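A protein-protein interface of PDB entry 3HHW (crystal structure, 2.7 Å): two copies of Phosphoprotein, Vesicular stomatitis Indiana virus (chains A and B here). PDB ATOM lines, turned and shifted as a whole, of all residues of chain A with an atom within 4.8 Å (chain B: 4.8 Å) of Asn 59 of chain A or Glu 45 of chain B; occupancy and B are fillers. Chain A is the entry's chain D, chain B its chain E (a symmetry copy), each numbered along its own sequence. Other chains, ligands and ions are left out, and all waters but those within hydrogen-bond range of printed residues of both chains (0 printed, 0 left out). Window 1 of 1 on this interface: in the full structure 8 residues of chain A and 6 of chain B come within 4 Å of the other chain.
ND2 of Asn 59 of chain A lies within hydrogen-bond range of O of Gly 57 of chain A (3.5 Å).
Hydrophobic or aromatic side chains of chain A within 4 Å of the printed part of chain B: Ile 54.
Of the 10 printed residues of chain B, 5 touch a printed residue of chain A.
Among the printed residues, no Asp or Glu carboxylate lies within 4 Å of a Lys or Arg side-chain nitrogen of the other chain.
The backbone NH (N) of Ser 55 of chain A is in hydrogen-bond range of the side-chain carboxylate (OE1) of Glu 45 of chain B (2.9 Å).
N of Val 56 of chain A sits at hydrogen-bond distance from OE1 of Glu 45 of chain B (3.3 Å).
N of Gly 57 of chain A sits at hydrogen-bond distance from OE1 of Glu 45 of chain B (2.8 Å).
OD1 of Asn 59 of chain A lies close to OE2 of Glu 45 of chain B (2.9 Å).
The guanidinium group (NH2) of Arg 61 of chain A is in hydrogen-bond range of the side-chain hydroxyl (OG) of Ser 26 of chain B (2.7 Å).
No position is printed for both chains.
Of the 12 pairs that touch across the chains among the printed residues, none has its exchanged pair printed and touching as well.
Ser 17 of chain A touches Lys 24 of chain B (OG to CE, 3.4 Å).
OD2 of Asp 44 of chain B touches CG2 of Ile 54 of chain A, at 3.4 Å.
OE2 of Glu 45 of chain B touches CG2 of Ile 54 of chain A, 3.4 Å away.
Glu 45 of chain B touches Gly 58 of chain A (OE2 to O, 3.7 Å).
Lys 24 of chain B touches Asn 59 of chain A (O to CB, 3.8 Å).
CB of Ser 26 of chain B touches ND2 of Asn 59 of chain A, at 3.5 Å.
ND2 of Asn 59 of chain A touches CB of Ser 42 of chain B, at 3.7 Å.
Of the printed residues of chain B, Ser 55 of chain A touches Glu 45.
Printed residues of chain B within 4 Å of Val 56 of chain A: Glu 45.
Of the printed residues of chain A, Lys 24 of chain B touches Ser 17 (3.4 Å) and Asn 59 (3.8 Å).
Of the printed residues of chain A, Ser 26 of chain B touches Asn 59 (3.5 Å) and Arg 61 (2.7 Å).
Glu 45 of chain B touches six residues of chain A.
The nearest residue of chain A that does not touch Glu 45 of chain B is Phe 53 of chain A (4.03 Å).
The nearest printed residue of chain B that does not touch Val 56 of chain A is Asp 44 of chain B (7.4 Å).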
ATOM      1  N   SER A  17      -7.756   6.866   6.123  1.00  0.00           N
ATOM      2  CA  SER A  17      -9.041   6.849   6.834  1.00  0.00           C
ATOM      3  C   SER A  17      -9.878   5.596   6.540  1.00  0.00           C
ATOM      4  O   SER A  17      -9.379   4.633   5.955  1.00  0.00           O
ATOM      5  CB  SER A  17      -9.841   8.116   6.509  1.00  0.00           C
ATOM      6  OG  SER A  17      -9.110   9.285   6.836  1.00  0.00           O
ATOM      7  N   VAL A  19     -11.997   4.535   4.429  1.00  0.00           N
ATOM      8  CA  VAL A  19     -12.074   3.970   3.079  1.00  0.00           C
ATOM      9  C   VAL A  19     -10.717   3.439   2.571  1.00  0.00           C
ATOM     10  O   VAL A  19     -10.671   2.661   1.615  1.00  0.00           O
ATOM     11  CB  VAL A  19     -12.726   4.970   2.076  1.00  0.00           C
ATOM     12  CG1 VAL A  19     -11.719   6.005   1.585  1.00  0.00           C
ATOM     13  CG2 VAL A  19     -13.369   4.232   0.905  1.00  0.00           C
ATOM     14  N   PHE A  53      -4.213  11.269  -2.046  1.00  0.00           N
ATOM     15  CA  PHE A  53      -5.578  10.901  -1.663  1.00  0.00           C
ATOM     16  C   PHE A  53      -6.301  12.043  -0.952  1.00  0.00           C
ATOM     17  O   PHE A  53      -7.478  12.297  -1.215  1.00  0.00           O
ATOM     18  CB  PHE A  53      -5.566   9.652  -0.777  1.00  0.00           C
ATOM     19  CG  PHE A  53      -6.892   8.943  -0.704  1.00  0.00           C
ATOM     20  CD1 PHE A  53      -7.247   8.006  -1.671  1.00  0.00           C
ATOM     21  CD2 PHE A  53      -7.782   9.202   0.334  1.00  0.00           C
ATOM     22  CE1 PHE A  53      -8.469   7.342  -1.609  1.00  0.00           C
ATOM     23  CE2 PHE A  53      -9.006   8.541   0.404  1.00  0.00           C
ATOM     24  CZ  PHE A  53      -9.350   7.612  -0.572  1.00  0.00           C
ATOM     25  N   ILE A  54      -5.591  12.719  -0.052  1.00  0.00           N
ATOM     26  CA  ILE A  54      -6.152  13.835   0.712  1.00  0.00           C
ATOM     27  C   ILE A  54      -5.820  15.167   0.022  1.00  0.00           C
ATOM     28  O   ILE A  54      -5.120  16.023   0.575  1.00  0.00           O
ATOM     29  CB  ILE A  54      -5.684  13.813   2.207  1.00  0.00           C
ATOM     30  CG1 ILE A  54      -5.746  12.391   2.799  1.00  0.00           C
ATOM     31  CG2 ILE A  54      -6.485  14.808   3.058  1.00  0.00           C
ATOM     32  CD1 ILE A  54      -7.145  11.775   2.913  1.00  0.00           C
ATOM     33  N   SER A  55      -6.322  15.312  -1.204  1.00  0.00           N
ATOM     34  CA  SER A  55      -6.172  16.525  -2.017  1.00  0.00           C
ATOM     35  C   SER A  55      -7.171  16.516  -3.173  1.00  0.00           C
ATOM     36  O   SER A  55      -7.570  17.573  -3.669  1.00  0.00           O
ATOM     37  CB  SER A  55      -4.748  16.651  -2.570  1.00  0.00           C
ATOM     38  OG  SER A  55      -3.830  17.024  -1.556  1.00  0.00           O
ATOM     39  N   VAL A  56      -7.571  15.314  -3.588  1.00  0.00           N
ATOM     40  CA  VAL A  56      -8.480  15.120  -4.721  1.00  0.00           C
ATOM     41  C   VAL A  56      -9.960  15.120  -4.322  1.00  0.00           C
ATOM     42  O   VAL A  56     -10.831  15.388  -5.151  1.00  0.00           O
ATOM     43  CB  VAL A  56      -8.156  13.818  -5.507  1.00  0.00           C
ATOM     44  CG1 VAL A  56      -6.820  13.940  -6.222  1.00  0.00           C
ATOM     45  CG2 VAL A  56      -8.170  12.591  -4.587  1.00  0.00           C
ATOM     46  N   GLY A  57     -10.234  14.815  -3.056  1.00  0.00           N
ATOM     47  CA  GLY A  57     -11.606  14.710  -2.565  1.00  0.00           C
ATOM     48  C   GLY A  57     -11.868  13.417  -1.816  1.00  0.00           C
ATOM     49  O   GLY A  57     -12.906  13.271  -1.166  1.00  0.00           O
ATOM     50  N   GLY A  58     -10.928  12.479  -1.912  1.00  0.00           N
ATOM     51  CA  GLY A  58     -11.018  11.206  -1.204  1.00  0.00           C
ATOM     52  C   GLY A  58     -10.794  11.382   0.285  1.00  0.00           C
ATOM     53  O   GLY A  58      -9.777  11.938   0.705  1.00  0.00           O
ATOM     54  N   ASN A  59     -11.751  10.908   1.078  1.00  0.00           N
ATOM     55  CA  ASN A  59     -11.689  11.035   2.533  1.00  0.00           C
ATOM     56  C   ASN A  59     -11.764   9.678   3.240  1.00  0.00           C
ATOM     57  O   ASN A  59     -10.748   8.994   3.389  1.00  0.00           O
ATOM     58  CB  ASN A  59     -12.787  11.982   3.040  1.00  0.00           C
ATOM     59  CG  ASN A  59     -12.735  13.353   2.380  1.00  0.00           C
ATOM     60  OD1 ASN A  59     -11.661  13.908   2.148  1.00  0.00           O
ATOM     61  ND2 ASN A  59     -13.904  13.905   2.079  1.00  0.00           N
ATOM     62  N   GLY A  60     -12.968   9.299   3.666  1.00  0.00           N
ATOM     63  CA  GLY A  60     -13.202   8.030   4.356  1.00  0.00           C
ATOM     64  C   GLY A  60     -14.680   7.712   4.477  1.00  0.00           C
ATOM     65  O   GLY A  60     -15.061   6.566   4.727  1.00  0.00           O
ATOM     66  N   ARG A  61     -15.508   8.739   4.292  1.00  0.00           N
ATOM     67  CA  ARG A  61     -16.961   8.629   4.391  1.00  0.00           C
ATOM     68  C   ARG A  61     -17.572   8.043   3.116  1.00  0.00           C
ATOM     69  O   ARG A  61     -18.723   7.597   3.117  1.00  0.00           O
ATOM     70  CB  ARG A  61     -17.553  10.012   4.674  1.00  0.00           C
ATOM     71  CG  ARG A  61     -18.895  10.005   5.384  1.00  0.00           C
ATOM     72  CD  ARG A  61     -19.270  11.407   5.838  1.00  0.00           C
ATOM     73  NE  ARG A  61     -19.563  12.296   4.713  1.00  0.00           N
ATOM     74  CZ  ARG A  61     -19.741  13.611   4.812  1.00  0.00           C
ATOM     75  NH1 ARG A  61     -19.655  14.219   5.989  1.00  0.00           N
ATOM     76  NH2 ARG A  61     -20.006  14.324   3.726  1.00  0.00           N
ATOM     77  N   LYS B  24     -11.792  15.976   8.440  1.00  0.00           N
ATOM     78  CA  LYS B  24     -12.060  14.683   7.807  1.00  0.00           C
ATOM     79  C   LYS B  24     -13.450  14.608   7.168  1.00  0.00           C
ATOM     80  O   LYS B  24     -13.607  14.050   6.079  1.00  0.00           O
ATOM     81  CB  LYS B  24     -11.862  13.546   8.812  1.00  0.00           C
ATOM     82  CG  LYS B  24     -11.523  12.202   8.176  1.00  0.00           C
ATOM     83  CD  LYS B  24     -10.688  11.331   9.107  1.00  0.00           C
ATOM     84  CE  LYS B  24      -9.232  11.785   9.149  1.00  0.00           C
ATOM     85  NZ  LYS B  24      -8.408  10.943  10.059  1.00  0.00           N
ATOM     86  N   SER B  26     -16.800  15.899   5.228  1.00  0.00           N
ATOM     87  CA  SER B  26     -16.960  16.730   4.033  1.00  0.00           C
ATOM     88  C   SER B  26     -18.341  17.381   3.922  1.00  0.00           C
ATOM     89  O   SER B  26     -19.315  16.910   4.515  1.00  0.00           O
ATOM     90  CB  SER B  26     -16.662  15.911   2.774  1.00  0.00           C
ATOM     91  OG  SER B  26     -17.531  14.797   2.668  1.00  0.00           O
ATOM     92  N   ILE B  41     -16.619  18.854  -0.746  1.00  0.00           N
ATOM     93  CA  ILE B  41     -15.408  19.513  -0.254  1.00  0.00           C
ATOM     94  C   ILE B  41     -15.148  19.232   1.231  1.00  0.00           C
ATOM     95  O   ILE B  41     -16.066  19.271   2.052  1.00  0.00           O
ATOM     96  CB  ILE B  41     -15.432  21.055  -0.555  1.00  0.00           C
ATOM     97  CG1 ILE B  41     -14.092  21.724  -0.209  1.00  0.00           C
ATOM     98  CG2 ILE B  41     -16.603  21.752   0.148  1.00  0.00           C
ATOM     99  CD1 ILE B  41     -13.002  21.515  -1.244  1.00  0.00           C
ATOM    100  N   SER B  42     -13.890  18.931   1.553  1.00  0.00           N
ATOM    101  CA  SER B  42     -13.444  18.758   2.935  1.00  0.00           C
ATOM    102  C   SER B  42     -12.347  19.775   3.266  1.00  0.00           C
ATOM    103  O   SER B  42     -11.746  20.360   2.362  1.00  0.00           O
ATOM    104  CB  SER B  42     -12.953  17.327   3.168  1.00  0.00           C
ATOM    105  OG  SER B  42     -12.666  17.099   4.538  1.00  0.00           O
ATOM    106  N   LEU B  43     -12.093  19.977   4.559  1.00  0.00           N
ATOM    107  CA  LEU B  43     -11.158  21.009   5.025  1.00  0.00           C
ATOM    108  C   LEU B  43      -9.687  20.777   4.668  1.00  0.00           C
ATOM    109  O   LEU B  43      -8.988  21.717   4.287  1.00  0.00           O
ATOM    110  CB  LEU B  43     -11.304  21.236   6.536  1.00  0.00           C
ATOM    111  CG  LEU B  43     -12.288  22.323   6.977  1.00  0.00           C
ATOM    112  CD1 LEU B  43     -12.561  22.237   8.470  1.00  0.00           C
ATOM    113  CD2 LEU B  43     -11.768  23.706   6.604  1.00  0.00           C
ATOM    114  N   ASP B  44      -9.227  19.533   4.788  1.00  0.00           N
ATOM    115  CA  ASP B  44      -7.821  19.199   4.535  1.00  0.00           C
ATOM    116  C   ASP B  44      -7.480  19.121   3.039  1.00  0.00           C
ATOM    117  O   ASP B  44      -6.309  19.004   2.667  1.00  0.00           O
ATOM    118  CB  ASP B  44      -7.437  17.897   5.253  1.00  0.00           C
ATOM    119  CG  ASP B  44      -5.938  17.785   5.514  1.00  0.00           C
ATOM    120  OD1 ASP B  44      -5.233  18.817   5.486  1.00  0.00           O
ATOM    121  OD2 ASP B  44      -5.464  16.654   5.755  1.00  0.00           O
ATOM    122  N   GLU B  45      -8.505  19.200   2.190  1.00  0.00           N
ATOM    123  CA  GLU B  45      -8.323  19.193   0.735  1.00  0.00           C
ATOM    124  C   GLU B  45      -7.868  20.561   0.215  1.00  0.00           C
ATOM    125  O   GLU B  45      -7.405  20.676  -0.923  1.00  0.00           O
ATOM    126  CB  GLU B  45      -9.615  18.766   0.023  1.00  0.00           C
ATOM    127  CG  GLU B  45     -10.317  17.537   0.613  1.00  0.00           C
ATOM    128  CD  GLU B  45      -9.542  16.241   0.427  1.00  0.00           C
ATOM    129  OE1 GLU B  45      -9.152  15.930  -0.717  1.00  0.00           O
ATOM    130  OE2 GLU B  45      -9.336  15.525   1.428  1.00  0.00           O
ATOM    131  N   LEU B  46      -8.004  21.585   1.055  1.00  0.00           N
ATOM    132  CA  LEU B  46      -7.626  22.954   0.697  1.00  0.00           C
ATOM    133  C   LEU B  46      -6.453  23.489   1.527  1.00  0.00           C
ATOM    134  O   LEU B  46      -6.085  24.659   1.404  1.00  0.00           O
ATOM    135  CB  LEU B  46      -8.834  23.895   0.825  1.00  0.00           C
ATOM    136  CG  LEU B  46     -10.023  23.720  -0.127  1.00  0.00           C
ATOM    137  CD1 LEU B  46     -11.232  24.484   0.394  1.00  0.00           C
ATOM    138  CD2 LEU B  46      -9.679  24.154  -1.550  1.00  0.00           C
ATOM    139  N   PHE B  47      -5.874  22.636   2.372  1.00  0.00           N
ATOM    140  CA  PHE B  47      -4.732  23.023   3.206  1.00  0.00           C
ATOM    141  C   PHE B  47      -3.663  21.934   3.266  1.00  0.00           C
ATOM    142  O   PHE B  47      -3.980  20.745   3.347  1.00  0.00           O
ATOM    143  CB  PHE B  47      -5.185  23.399   4.623  1.00  0.00           C
ATOM    144  CG  PHE B  47      -6.114  24.584   4.675  1.00  0.00           C
ATOM    145  CD1 PHE B  47      -5.649  25.868   4.395  1.00  0.00           C
ATOM    146  CD2 PHE B  47      -7.452  24.418   5.013  1.00  0.00           C
ATOM    147  CE1 PHE B  47      -6.507  26.964   4.444  1.00  0.00           C
ATOM    148  CE2 PHE B  47      -8.319  25.507   5.067  1.00  0.00           C
ATOM    149  CZ  PHE B  47      -7.844  26.783   4.782  1.00  0.00           C
ATOM    150  N   TYR B  74      -6.424  27.818  -1.960  1.00  0.00           N
ATOM    151  CA  TYR B  74      -5.434  26.826  -2.387  1.00  0.00           C
ATOM    152  C   TYR B  74      -5.732  26.304  -3.789  1.00  0.00           C
ATOM    153  O   TYR B  74      -4.814  26.050  -4.575  1.00  0.00           O
ATOM    154  CB  TYR B  74      -5.378  25.667  -1.386  1.00  0.00           C
ATOM    155  CG  TYR B  74      -4.509  24.498  -1.807  1.00  0.00           C
ATOM    156  CD1 TYR B  74      -5.078  23.327  -2.306  1.00  0.00           C
ATOM    157  CD2 TYR B  74      -3.119  24.564  -1.702  1.00  0.00           C
ATOM    158  CE1 TYR B  74      -4.285  22.250  -2.695  1.00  0.00           C
ATOM    159  CE2 TYR B  74      -2.317  23.493  -2.087  1.00  0.00           C
ATOM    160  CZ  TYR B  74      -2.907  22.340  -2.582  1.00  0.00           C
ATOM    161  OH  TYR B  74      -2.121  21.277  -2.965  1.00  0.00           O
